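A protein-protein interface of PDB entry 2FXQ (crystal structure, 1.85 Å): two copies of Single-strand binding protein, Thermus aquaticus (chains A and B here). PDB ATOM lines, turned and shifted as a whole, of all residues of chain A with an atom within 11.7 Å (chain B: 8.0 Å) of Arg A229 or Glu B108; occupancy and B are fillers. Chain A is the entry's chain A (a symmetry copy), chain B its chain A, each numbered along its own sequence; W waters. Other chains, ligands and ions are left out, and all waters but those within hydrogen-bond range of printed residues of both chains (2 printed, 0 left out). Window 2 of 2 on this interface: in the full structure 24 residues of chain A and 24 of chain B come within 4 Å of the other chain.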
ATOM      1  N   ARG A   3      23.663 -11.535  -5.253  1.00  0.00           N
ATOM      2  CA  ARG A   3      22.874 -12.587  -5.947  1.00  0.00           C
ATOM      3  C   ARG A   3      23.311 -13.951  -5.420  1.00  0.00           C
ATOM      4  O   ARG A   3      24.470 -14.119  -5.004  1.00  0.00           O
ATOM      5  CB  ARG A   3      23.106 -12.497  -7.456  1.00  0.00           C
ATOM      6  N   GLY A   4      22.416 -14.929  -5.421  1.00  0.00           N
ATOM      7  CA  GLY A   4      22.807 -16.260  -4.997  1.00  0.00           C
ATOM      8  C   GLY A   4      23.826 -16.932  -5.918  1.00  0.00           C
ATOM      9  O   GLY A   4      23.938 -16.581  -7.106  1.00  0.00           O
ATOM     10  N   MET A 134      26.572 -18.947  -2.418  1.00  0.00           N
ATOM     11  CA  MET A 134      26.403 -17.669  -1.725  1.00  0.00           C
ATOM     12  C   MET A 134      24.923 -17.545  -1.467  1.00  0.00           C
ATOM     13  O   MET A 134      24.085 -17.720  -2.410  1.00  0.00           O
ATOM     14  CB  MET A 134      26.849 -16.495  -2.587  1.00  0.00           C
ATOM     15  CG  MET A 134      27.009 -15.146  -1.671  1.00  0.00           C
ATOM     16  SD  MET A 134      27.738 -13.895  -2.668  1.00  0.00           S
ATOM     17  CE  MET A 134      29.428 -14.031  -2.367  1.00  0.00           C
ATOM     18  N   GLY A 135      24.570 -17.210  -0.226  1.00  0.00           N
ATOM     19  CA  GLY A 135      23.135 -17.116   0.101  1.00  0.00           C
ATOM     20  C   GLY A 135      22.948 -16.452   1.469  1.00  0.00           C
ATOM     21  O   GLY A 135      23.784 -15.633   1.860  1.00  0.00           O
ATOM     22  N   ASN A 136      21.862 -16.759   2.155  1.00  0.00           N
ATOM     23  CA  ASN A 136      21.567 -16.103   3.472  1.00  0.00           C
ATOM     24  C   ASN A 136      21.176 -17.166   4.428  1.00  0.00           C
ATOM     25  O   ASN A 136      20.483 -18.120   4.039  1.00  0.00           O
ATOM     26  CB  ASN A 136      20.429 -15.105   3.355  1.00  0.00           C
ATOM     27  CG  ASN A 136      20.847 -13.884   2.494  1.00  0.00           C
ATOM     28  OD1 ASN A 136      20.747 -13.914   1.267  1.00  0.00           O
ATOM     29  ND2 ASN A 136      21.372 -12.866   3.144  1.00  0.00           N
ATOM     30  N   LEU A 137      21.645 -17.049   5.669  1.00  0.00           N
ATOM     31  CA  LEU A 137      21.310 -18.085   6.674  1.00  0.00           C
ATOM     32  C   LEU A 137      19.784 -18.150   6.931  1.00  0.00           C
ATOM     33  O   LEU A 137      19.122 -17.127   7.062  1.00  0.00           O
ATOM     34  CB  LEU A 137      22.077 -17.818   7.971  1.00  0.00           C
ATOM     35  CG  LEU A 137      23.592 -18.072   8.012  1.00  0.00           C
ATOM     36  CD1 LEU A 137      23.936 -17.975   9.486  1.00  0.00           C
ATOM     37  CD2 LEU A 137      23.926 -19.481   7.506  1.00  0.00           C
ATOM     38  N   TRP A 185      33.983 -19.269  14.345  1.00  0.00           N
ATOM     39  CA  TRP A 185      33.688 -18.005  13.654  1.00  0.00           C
ATOM     40  C   TRP A 185      32.236 -17.948  13.161  1.00  0.00           C
ATOM     41  O   TRP A 185      31.564 -16.933  13.329  1.00  0.00           O
ATOM     42  CB  TRP A 185      34.648 -17.861  12.460  1.00  0.00           C
ATOM     43  CG  TRP A 185      34.400 -16.648  11.660  1.00  0.00           C
ATOM     44  CD1 TRP A 185      34.951 -15.381  11.855  1.00  0.00           C
ATOM     45  CD2 TRP A 185      33.532 -16.542  10.516  1.00  0.00           C
ATOM     46  NE1 TRP A 185      34.464 -14.527  10.888  1.00  0.00           N
ATOM     47  CE2 TRP A 185      33.601 -15.204  10.061  1.00  0.00           C
ATOM     48  CE3 TRP A 185      32.716 -17.451   9.824  1.00  0.00           C
ATOM     49  CZ2 TRP A 185      32.863 -14.751   8.963  1.00  0.00           C
ATOM     50  CZ3 TRP A 185      31.971 -17.017   8.795  1.00  0.00           C
ATOM     51  CH2 TRP A 185      32.068 -15.660   8.327  1.00  0.00           C
ATOM     52  N   GLU A 188      29.107 -16.654  15.138  1.00  0.00           N
ATOM     53  CA  GLU A 188      28.775 -15.222  15.341  1.00  0.00           C
ATOM     54  C   GLU A 188      27.690 -14.755  14.371  1.00  0.00           C
ATOM     55  O   GLU A 188      27.191 -13.657  14.506  1.00  0.00           O
ATOM     56  CB  GLU A 188      29.994 -14.296  15.104  1.00  0.00           C
ATOM     57  CG  GLU A 188      31.310 -14.673  15.766  1.00  0.00           C
ATOM     58  CD  GLU A 188      32.543 -14.288  14.912  1.00  0.00           C
ATOM     59  OE1 GLU A 188      32.399 -14.007  13.678  1.00  0.00           O
ATOM     60  OE2 GLU A 188      33.672 -14.265  15.477  1.00  0.00           O
ATOM     61  N   LEU A 189      27.392 -15.565  13.353  1.00  0.00           N
ATOM     62  CA  LEU A 189      26.395 -15.196  12.345  1.00  0.00           C
ATOM     63  C   LEU A 189      24.979 -15.404  12.926  1.00  0.00           C
ATOM     64  O   LEU A 189      24.852 -16.058  13.950  1.00  0.00           O
ATOM     65  CB  LEU A 189      26.597 -16.112  11.135  1.00  0.00           C
ATOM     66  CG  LEU A 189      27.972 -16.131  10.371  1.00  0.00           C
ATOM     67  CD1 LEU A 189      28.152 -17.452   9.545  1.00  0.00           C
ATOM     68  CD2 LEU A 189      27.977 -14.974   9.452  1.00  0.00           C
ATOM     69  N   ARG A 190      23.942 -14.891  12.258  1.00  0.00           N
ATOM     70  CA  ARG A 190      22.559 -14.990  12.747  1.00  0.00           C
ATOM     71  C   ARG A 190      21.670 -15.193  11.539  1.00  0.00           C
ATOM     72  O   ARG A 190      22.081 -14.896  10.435  1.00  0.00           O
ATOM     73  CB  ARG A 190      22.195 -13.669  13.447  1.00  0.00           C
ATOM     74  CG  ARG A 190      22.978 -13.382  14.776  1.00  0.00           C
ATOM     75  CD  ARG A 190      22.634 -14.367  15.926  1.00  0.00           C
ATOM     76  NE  ARG A 190      23.308 -14.079  17.193  1.00  0.00           N
ATOM     77  CZ  ARG A 190      24.506 -14.564  17.549  1.00  0.00           C
ATOM     78  NH1 ARG A 190      25.162 -15.389  16.740  1.00  0.00           N
ATOM     79  NH2 ARG A 190      25.055 -14.232  18.719  1.00  0.00           N
ATOM     80  N   LYS A 191      20.446 -15.666  11.755  1.00  0.00           N
ATOM     81  CA  LYS A 191      19.497 -15.882  10.683  1.00  0.00           C
ATOM     82  C   LYS A 191      19.425 -14.616   9.844  1.00  0.00           C
ATOM     83  O   LYS A 191      19.435 -13.492  10.403  1.00  0.00           O
ATOM     84  CB  LYS A 191      18.101 -16.187  11.336  1.00  0.00           C
ATOM     85  CG  LYS A 191      16.915 -16.152  10.385  1.00  0.00           C
ATOM     86  CD  LYS A 191      15.581 -16.262  11.213  1.00  0.00           C
ATOM     87  CE  LYS A 191      14.545 -16.990  10.410  1.00  0.00           C
ATOM     88  NZ  LYS A 191      13.225 -16.904  11.125  1.00  0.00           N
ATOM     89  N   GLY A 192      19.420 -14.770   8.524  1.00  0.00           N
ATOM     90  CA  GLY A 192      19.388 -13.619   7.635  1.00  0.00           C
ATOM     91  C   GLY A 192      20.722 -13.183   7.058  1.00  0.00           C
ATOM     92  O   GLY A 192      20.731 -12.603   5.978  1.00  0.00           O
ATOM     93  N   ASP A 193      21.838 -13.458   7.745  1.00  0.00           N
ATOM     94  CA  ASP A 193      23.152 -12.937   7.319  1.00  0.00           C
ATOM     95  C   ASP A 193      23.532 -13.577   5.981  1.00  0.00           C
ATOM     96  O   ASP A 193      23.282 -14.764   5.734  1.00  0.00           O
ATOM     97  CB  ASP A 193      24.224 -13.268   8.399  1.00  0.00           C
ATOM     98  CG  ASP A 193      24.121 -12.372   9.617  1.00  0.00           C
ATOM     99  OD1 ASP A 193      24.790 -12.688  10.650  1.00  0.00           O
ATOM    100  OD2 ASP A 193      23.419 -11.319   9.603  1.00  0.00           O
ATOM    101  N   GLY A 194      24.176 -12.798   5.127  1.00  0.00           N
ATOM    102  CA  GLY A 194      24.725 -13.289   3.880  1.00  0.00           C
ATOM    103  C   GLY A 194      26.011 -14.069   4.196  1.00  0.00           C
ATOM    104  O   GLY A 194      26.743 -13.810   5.189  1.00  0.00           O
ATOM    105  N   LEU A 195      26.259 -15.071   3.364  1.00  0.00           N
ATOM    106  CA  LEU A 195      27.401 -15.935   3.542  1.00  0.00           C
ATOM    107  C   LEU A 195      27.883 -16.429   2.184  1.00  0.00           C
ATOM    108  O   LEU A 195      27.091 -16.963   1.392  1.00  0.00           O
ATOM    109  CB  LEU A 195      27.001 -17.124   4.412  1.00  0.00           C
ATOM    110  CG  LEU A 195      28.144 -18.032   4.871  1.00  0.00           C
ATOM    111  CD1 LEU A 195      29.171 -17.222   5.711  1.00  0.00           C
ATOM    112  CD2 LEU A 195      27.575 -19.257   5.651  1.00  0.00           C
ATOM    113  N   LEU A 196      29.211 -16.344   1.962  1.00  0.00           N
ATOM    114  CA  LEU A 196      29.869 -17.038   0.834  1.00  0.00           C
ATOM    115  C   LEU A 196      30.578 -18.293   1.358  1.00  0.00           C
ATOM    116  O   LEU A 196      31.314 -18.209   2.353  1.00  0.00           O
ATOM    117  CB  LEU A 196      30.917 -16.070   0.240  1.00  0.00           C
ATOM    118  CG  LEU A 196      31.899 -16.674  -0.824  1.00  0.00           C
ATOM    119  CD1 LEU A 196      31.098 -17.101  -2.078  1.00  0.00           C
ATOM    120  CD2 LEU A 196      32.936 -15.634  -1.234  1.00  0.00           C
ATOM    121  N   VAL A 197      30.331 -19.456   0.748  1.00  0.00           N
ATOM    122  CA  VAL A 197      30.981 -20.673   1.227  1.00  0.00           C
ATOM    123  C   VAL A 197      31.839 -21.203   0.083  1.00  0.00           C
ATOM    124  O   VAL A 197      31.334 -21.317  -1.035  1.00  0.00           O
ATOM    125  CB  VAL A 197      29.952 -21.689   1.439  1.00  0.00           C
ATOM    126  CG1 VAL A 197      30.535 -23.085   1.926  1.00  0.00           C
ATOM    127  CG2 VAL A 197      28.859 -21.157   2.495  1.00  0.00           C
ATOM    128  N   ARG A 223      36.175 -22.526   3.421  1.00  0.00           N
ATOM    129  CA  ARG A 223      36.386 -21.100   3.667  1.00  0.00           C
ATOM    130  C   ARG A 223      34.992 -20.502   3.797  1.00  0.00           C
ATOM    131  O   ARG A 223      34.056 -20.942   3.125  1.00  0.00           O
ATOM    132  CB  ARG A 223      37.038 -20.448   2.445  1.00  0.00           C
ATOM    133  CG  ARG A 223      37.380 -18.980   2.710  1.00  0.00           C
ATOM    134  CD  ARG A 223      38.519 -18.432   1.835  1.00  0.00           C
ATOM    135  NE  ARG A 223      38.702 -16.998   2.060  1.00  0.00           N
ATOM    136  CZ  ARG A 223      39.701 -16.256   1.534  1.00  0.00           C
ATOM    137  NH1 ARG A 223      40.647 -16.772   0.783  1.00  0.00           N
ATOM    138  NH2 ARG A 223      39.760 -14.979   1.774  1.00  0.00           N
ATOM    139  N   LEU A 224      34.838 -19.515   4.677  1.00  0.00           N
ATOM    140  CA  LEU A 224      33.601 -18.779   4.778  1.00  0.00           C
ATOM    141  C   LEU A 224      33.937 -17.265   4.810  1.00  0.00           C
ATOM    142  O   LEU A 224      34.897 -16.838   5.453  1.00  0.00           O
ATOM    143  CB  LEU A 224      32.883 -19.097   6.142  1.00  0.00           C
ATOM    144  CG  LEU A 224      32.402 -20.551   6.339  1.00  0.00           C
ATOM    145  CD1 LEU A 224      31.805 -20.666   7.753  1.00  0.00           C
ATOM    146  CD2 LEU A 224      31.374 -20.879   5.282  1.00  0.00           C
ATOM    147  N   GLU A 225      33.150 -16.475   4.098  1.00  0.00           N
ATOM    148  CA  GLU A 225      33.348 -15.047   4.065  1.00  0.00           C
ATOM    149  C   GLU A 225      31.963 -14.426   4.089  1.00  0.00           C
ATOM    150  O   GLU A 225      30.995 -15.064   3.737  1.00  0.00           O
ATOM    151  CB  GLU A 225      34.092 -14.578   2.792  1.00  0.00           C
ATOM    152  CG  GLU A 225      35.497 -15.165   2.587  1.00  0.00           C
ATOM    153  CD  GLU A 225      36.506 -14.709   3.650  1.00  0.00           C
ATOM    154  OE1 GLU A 225      37.586 -15.350   3.811  1.00  0.00           O
ATOM    155  OE2 GLU A 225      36.222 -13.722   4.369  1.00  0.00           O
ATOM    156  N   ARG A 226      31.907 -13.153   4.468  1.00  0.00           N
ATOM    157  CA  ARG A 226      30.679 -12.407   4.446  1.00  0.00           C
ATOM    158  C   ARG A 226      30.617 -11.379   3.305  1.00  0.00           C
ATOM    159  O   ARG A 226      31.430 -10.453   3.256  1.00  0.00           O
ATOM    160  CB  ARG A 226      30.616 -11.618   5.758  1.00  0.00           C
ATOM    161  CG  ARG A 226      30.650 -12.469   6.996  1.00  0.00           C
ATOM    162  CD  ARG A 226      30.462 -11.641   8.252  1.00  0.00           C
ATOM    163  NE  ARG A 226      29.064 -11.251   8.363  1.00  0.00           N
ATOM    164  CZ  ARG A 226      28.487 -10.965   9.517  1.00  0.00           C
ATOM    165  NH1 ARG A 226      29.211 -11.029  10.636  1.00  0.00           N
ATOM    166  NH2 ARG A 226      27.204 -10.637   9.556  1.00  0.00           N
ATOM    167  N   PRO A 227      29.640 -11.490   2.422  1.00  0.00           N
ATOM    168  CA  PRO A 227      29.483 -10.527   1.338  1.00  0.00           C
ATOM    169  C   PRO A 227      29.041  -9.196   1.958  1.00  0.00           C
ATOM    170  O   PRO A 227      28.384  -9.183   2.996  1.00  0.00           O
ATOM    171  CB  PRO A 227      28.371 -11.123   0.478  1.00  0.00           C
ATOM    172  CG  PRO A 227      27.636 -12.042   1.402  1.00  0.00           C
ATOM    173  CD  PRO A 227      28.627 -12.573   2.372  1.00  0.00           C
ATOM    174  N   THR A 228      29.499  -8.105   1.414  1.00  0.00           N
ATOM    175  CA  THR A 228      29.011  -6.822   1.926  1.00  0.00           C
ATOM    176  C   THR A 228      27.459  -6.755   1.809  1.00  0.00           C
ATOM    177  O   THR A 228      26.892  -7.245   0.830  1.00  0.00           O
ATOM    178  CB  THR A 228      29.746  -5.685   1.188  1.00  0.00           C
ATOM    179  OG1 THR A 228      31.148  -5.796   1.489  1.00  0.00           O
ATOM    180  CG2 THR A 228      29.401  -4.348   1.792  1.00  0.00           C
ATOM    181  N   ARG A 229      26.812  -6.218   2.853  1.00  0.00           N
ATOM    182  CA  ARG A 229      25.352  -5.949   2.991  1.00  0.00           C
ATOM    183  C   ARG A 229      24.818  -6.321   4.389  1.00  0.00           C
ATOM    184  O   ARG A 229      23.648  -6.083   4.749  1.00  0.00           O
ATOM    185  CB  ARG A 229      24.494  -6.589   1.892  1.00  0.00           C
ATOM    186  CG  ARG A 229      23.454  -5.682   1.286  1.00  0.00           C
ATOM    187  CD  ARG A 229      23.976  -4.810   0.156  1.00  0.00           C
ATOM    188  NE  ARG A 229      25.274  -4.206   0.476  1.00  0.00           N
ATOM    189  CZ  ARG A 229      25.849  -3.228  -0.227  1.00  0.00           C
ATOM    190  NH1 ARG A 229      25.252  -2.736  -1.312  1.00  0.00           N
ATOM    191  NH2 ARG A 229      27.029  -2.744   0.146  1.00  0.00           N
ATOM    192  N   MET B  65      27.927  -0.434 -11.002  1.00  0.00           N
ATOM    193  CA  MET B  65      27.397  -0.967  -9.726  1.00  0.00           C
ATOM    194  C   MET B  65      28.352  -0.716  -8.563  1.00  0.00           C
ATOM    195  O   MET B  65      27.954  -0.295  -7.464  1.00  0.00           O
ATOM    196  CB  MET B  65      27.210  -2.490  -9.845  1.00  0.00           C
ATOM    197  CG  MET B  65      26.518  -3.097  -8.640  1.00  0.00           C
ATOM    198  SD  MET B  65      26.251  -4.881  -8.857  1.00  0.00           S
ATOM    199  CE  MET B  65      25.896  -4.993 -10.799  1.00  0.00           C
ATOM    200  N   TRP B  66      29.620  -1.020  -8.794  1.00  0.00           N
ATOM    201  CA  TRP B  66      30.615  -0.963  -7.716  1.00  0.00           C
ATOM    202  C   TRP B  66      31.538   0.240  -7.723  1.00  0.00           C
ATOM    203  O   TRP B  66      32.384   0.326  -6.869  1.00  0.00           O
ATOM    204  CB  TRP B  66      31.507  -2.213  -7.740  1.00  0.00           C
ATOM    205  CG  TRP B  66      30.726  -3.439  -7.647  1.00  0.00           C
ATOM    206  CD1 TRP B  66      30.520  -4.372  -8.603  1.00  0.00           C
ATOM    207  CD2 TRP B  66      30.020  -3.875  -6.493  1.00  0.00           C
ATOM    208  NE1 TRP B  66      29.713  -5.382  -8.112  1.00  0.00           N
ATOM    209  CE2 TRP B  66      29.406  -5.093  -6.808  1.00  0.00           C
ATOM    210  CE3 TRP B  66      29.877  -3.362  -5.200  1.00  0.00           C
ATOM    211  CZ2 TRP B  66      28.610  -5.798  -5.880  1.00  0.00           C
ATOM    212  CZ3 TRP B  66      29.123  -4.075  -4.269  1.00  0.00           C
ATOM    213  CH2 TRP B  66      28.481  -5.263  -4.623  1.00  0.00           C
ATOM    214  N   LEU B  69      32.053   2.146  -4.297  1.00  0.00           N
ATOM    215  CA  LEU B  69      31.777   1.383  -3.105  1.00  0.00           C
ATOM    216  C   LEU B  69      32.983   0.657  -2.559  1.00  0.00           C
ATOM    217  O   LEU B  69      32.899   0.138  -1.409  1.00  0.00           O
ATOM    218  CB  LEU B  69      30.657   0.373  -3.349  1.00  0.00           C
ATOM    219  CG  LEU B  69      29.312   1.056  -3.627  1.00  0.00           C
ATOM    220  CD1 LEU B  69      28.258   0.013  -4.007  1.00  0.00           C
ATOM    221  CD2 LEU B  69      28.874   1.915  -2.386  1.00  0.00           C
ATOM    222  N   GLY B  73      42.493  -2.373   0.495  1.00  0.00           N
ATOM    223  CA  GLY B  73      42.508  -3.220   1.686  1.00  0.00           C
ATOM    224  C   GLY B  73      41.319  -4.184   1.744  1.00  0.00           C
ATOM    225  O   GLY B  73      41.307  -5.116   2.537  1.00  0.00           O
ATOM    226  N   GLN B  74      40.309  -3.956   0.913  1.00  0.00           N
ATOM    227  CA  GLN B  74      39.094  -4.756   0.977  1.00  0.00           C
ATOM    228  C   GLN B  74      39.303  -6.050   0.227  1.00  0.00           C
ATOM    229  O   GLN B  74      39.881  -6.058  -0.869  1.00  0.00           O
ATOM    230  CB  GLN B  74      37.913  -4.019   0.287  1.00  0.00           C
ATOM    231  CG  GLN B  74      36.521  -4.743   0.517  1.00  0.00           C
ATOM    232  CD  GLN B  74      35.339  -3.839   0.151  1.00  0.00           C
ATOM    233  OE1 GLN B  74      35.531  -2.747  -0.383  1.00  0.00           O
ATOM    234  NE2 GLN B  74      34.113  -4.319   0.415  1.00  0.00           N
ATOM    235  N   LEU B  75      38.766  -7.115   0.781  1.00  0.00           N
ATOM    236  CA  LEU B  75      38.732  -8.437   0.128  1.00  0.00           C
ATOM    237  C   LEU B  75      37.597  -8.473  -0.892  1.00  0.00           C
ATOM    238  O   LEU B  75      36.465  -8.017  -0.609  1.00  0.00           O
ATOM    239  CB  LEU B  75      38.449  -9.487   1.204  1.00  0.00           C
ATOM    240  CG  LEU B  75      39.083 -10.849   1.257  1.00  0.00           C
ATOM    241  CD1 LEU B  75      40.617 -10.734   1.206  1.00  0.00           C
ATOM    242  CD2 LEU B  75      38.599 -11.553   2.587  1.00  0.00           C
ATOM    243  N   ILE B  76      37.886  -9.086  -2.045  1.00  0.00           N
ATOM    244  CA  ILE B  76      36.942  -9.142  -3.154  1.00  0.00           C
ATOM    245  C   ILE B  76      36.954 -10.580  -3.693  1.00  0.00           C
ATOM    246  O   ILE B  76      38.009 -11.170  -3.929  1.00  0.00           O
ATOM    247  CB  ILE B  76      37.338  -8.163  -4.306  1.00  0.00           C
ATOM    248  CG1 ILE B  76      37.621  -6.719  -3.828  1.00  0.00           C
ATOM    249  CG2 ILE B  76      36.331  -8.194  -5.416  1.00  0.00           C
ATOM    250  CD1 ILE B  76      36.372  -5.918  -3.312  1.00  0.00           C
ATOM    251  N   ASP B 105      31.939  -9.879  -5.827  1.00  0.00           N
ATOM    252  CA  ASP B 105      31.181  -9.700  -4.570  1.00  0.00           C
ATOM    253  C   ASP B 105      32.204  -9.252  -3.564  1.00  0.00           C
ATOM    254  O   ASP B 105      33.067 -10.030  -3.138  1.00  0.00           O
ATOM    255  CB  ASP B 105      30.581 -11.042  -4.125  1.00  0.00           C
ATOM    256  CG  ASP B 105      29.405 -11.485  -4.978  1.00  0.00           C
ATOM    257  OD1 ASP B 105      29.490 -12.575  -5.594  1.00  0.00           O
ATOM    258  OD2 ASP B 105      28.338 -10.837  -5.062  1.00  0.00           O
ATOM    259  N   PRO B 106      32.204  -7.973  -3.210  1.00  0.00           N
ATOM    260  CA  PRO B 106      33.060  -7.476  -2.156  1.00  0.00           C
ATOM    261  C   PRO B 106      32.732  -8.164  -0.837  1.00  0.00           C
ATOM    262  O   PRO B 106      31.558  -8.487  -0.590  1.00  0.00           O
ATOM    263  CB  PRO B 106      32.651  -5.975  -2.096  1.00  0.00           C
ATOM    264  CG  PRO B 106      32.067  -5.701  -3.399  1.00  0.00           C
ATOM    265  CD  PRO B 106      31.361  -6.906  -3.817  1.00  0.00           C
ATOM    266  N   LEU B 107      33.703  -8.338   0.040  1.00  0.00           N
ATOM    267  CA  LEU B 107      33.529  -9.142   1.224  1.00  0.00           C
ATOM    268  C   LEU B 107      33.866  -8.252   2.400  1.00  0.00           C
ATOM    269  O   LEU B 107      34.591  -7.257   2.218  1.00  0.00           O
ATOM    270  CB  LEU B 107      34.472 -10.326   1.243  1.00  0.00           C
ATOM    271  CG  LEU B 107      34.361 -11.167  -0.044  1.00  0.00           C
ATOM    272  CD1 LEU B 107      35.440 -12.315  -0.049  1.00  0.00           C
ATOM    273  CD2 LEU B 107      32.947 -11.841  -0.032  1.00  0.00           C
ATOM    274  N   GLU B 108      33.334  -8.599   3.585  1.00  0.00           N
ATOM    275  CA  GLU B 108      33.636  -7.857   4.802  1.00  0.00           C
ATOM    276  C   GLU B 108      35.011  -8.089   5.363  1.00  0.00           C
ATOM    277  O   GLU B 108      35.617  -7.169   5.918  1.00  0.00           O
ATOM    278  CB  GLU B 108      32.560  -8.110   5.838  1.00  0.00           C
ATOM    279  CG  GLU B 108      31.290  -7.479   5.309  1.00  0.00           C
ATOM    280  CD  GLU B 108      30.088  -7.694   6.212  1.00  0.00           C
ATOM    281  OE1 GLU B 108      28.958  -7.396   5.758  1.00  0.00           O
ATOM    282  OE2 GLU B 108      30.272  -8.138   7.365  1.00  0.00           O
ATOM    283  N   GLY B 109      35.528  -9.290   5.221  1.00  0.00           N
ATOM    284  CA  GLY B 109      36.976  -9.499   5.335  1.00  0.00           C
ATOM    285  C   GLY B 109      37.593  -8.965   6.634  1.00  0.00           C
ATOM    286  O   GLY B 109      38.715  -8.417   6.637  1.00  0.00           O
ATOM    287  N   ARG B 110      36.834  -9.114   7.725  1.00  0.00           N
ATOM    288  CA  ARG B 110      37.234  -8.671   9.057  1.00  0.00           C
ATOM    289  C   ARG B 110      37.772  -9.828   9.936  1.00  0.00           C
ATOM    290  O   ARG B 110      38.505 -10.721   9.467  1.00  0.00           O
ATOM    291  CB  ARG B 110      36.050  -7.968   9.743  1.00  0.00           C
HETATM  292  O   HOH W   1      34.411 -11.785   5.069  1.00  0.00           O
HETATM  293  O   HOH W   2      28.984  -8.502  -1.929  1.00  0.00           O
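The side-chain sulfur (SD) of Met A134 sits close to the side-chain carboxylate (OD1) of Asp B105 (3.7 Å).
The backbone NH (N) of Thr A228 sits at hydrogen-bond distance from the backbone carbonyl oxygen (O) of Pro B106 (2.9 Å).
The side-chain carboxylate (OE1) of Glu B108 sits close to the backbone carbonyl oxygen (O) of Pro A227 (3.3 Å).
The side-chain carboxylate of Glu B108 lies within salt-bridge range of the guanidinium group of Arg A226 (3.5 Å).
The side-chain amide nitrogen of Gln B74 is in hydrogen-bond range of the side-chain hydroxyl of Thr A228.
Along chain B the printed residues that touch a printed residue of chain A span positions 74 to 108.
Of the 24 printed residues of chain A, 8 touch a printed residue of chain B.
Hydrophobic or aromatic side chains of chain A that line the printed part of chain B: Met A134 and Leu A196.
Along chain A the printed residues that touch a printed residue of chain B span positions 134 to 229.
Among the printed residues, 15 pairs touch across the chains.
Among the printed residues, Asp or Glu carboxylates within 4 Å of a Lys or Arg side-chain nitrogen of the other chain: Arg A226 with Glu B108 (3.5 Å).
CD2 of Leu A196 touches CD2 of Leu B107 (3.98 Å).
Arg A223 touches Leu B75 (NH2 to CD2, 3.7 Å).
Glu A225 touches Leu B75 (OE2 to CD2, 3.7 Å).
Leu B107 touches Glu A225 (CD1 to CB, 3.9 Å).
CA of Leu B107 touches O of Arg A226, at 3.2 Å.
Pro A227 touches Pro B106 (CA to O, 3.5 Å).
Pro A227 touches Leu B107 (CA to CD2, 3.95 Å).
C of Leu B107 touches OG1 of Thr A228, 3.8 Å away.
Thr A228 touches Glu B108.
N of Arg A229 touches OE1 of Glu B108, 3.8 Å away.
Water W1 lies within hydrogen-bond range of N of Gly B109 (2.7 Å), OE2 of Glu A225 (2.7 Å) and N of Arg A226 (2.9 Å).
Water W2 bridges O of Pro B106 (2.9 Å) and N of Thr A228 (3.4 Å).
NE2 of Gln B74 lies within hydrogen-bond range of O of Leu B107 (3.5 Å).
The backbone carbonyl oxygen (O) of Leu B75 lies within hydrogen-bond range of the backbone NH (N) of Leu B107 (2.9 Å).
The side-chain carboxylate (OE1) of Glu A225 is in salt-bridge range of the guanidinium group (NE) of Arg A223, at 2.7 Å.
OD1 of Asp A193 lies within salt-bridge range of NH2 of Arg A226, 3.4 Å away.
The backbone NH (N) of Leu A196 is in hydrogen-bond range of the backbone carbonyl oxygen (O) of Glu A225 (2.8 Å).
No position is printed for both chains.
Of the 15 pairs that touch across the chains among the printed residues, none has its exchanged pair printed and touching as well.
Of the printed residues of chain B, Met A134 touches Asp B105.
Asn A136 touches none of the printed residues of chain B.
Leu A137 touches none of the printed residues of chain B.
Of the printed residues of chain B, Leu A196 touches Leu B107.
Of the printed residues of chain B, Arg A223 touches Leu B75 (3.7 Å).
Printed residues of chain B within 4 Å of Arg A226: Leu B107 and Glu B108.
Of chain A, only Arg A223 and Glu A225 come within 4 Å of Leu B75.
Of the printed residues of chain A, Asp B105 touches Met A134 (3.5 Å).
Pro B106 touches just these residues of chain A: Pro A227 and Thr A228.
Of chain A, only Arg A226, Pro A227, Thr A228 and Arg A229 come within 4 Å of Glu B108.
No residue of chain A comes within 4 Å of Gly B109.
Arg B110 touches none of the printed residues of chain A.
The nearest residue of chain A that does not touch Glu B108 is Glu A225 (5.8 Å).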
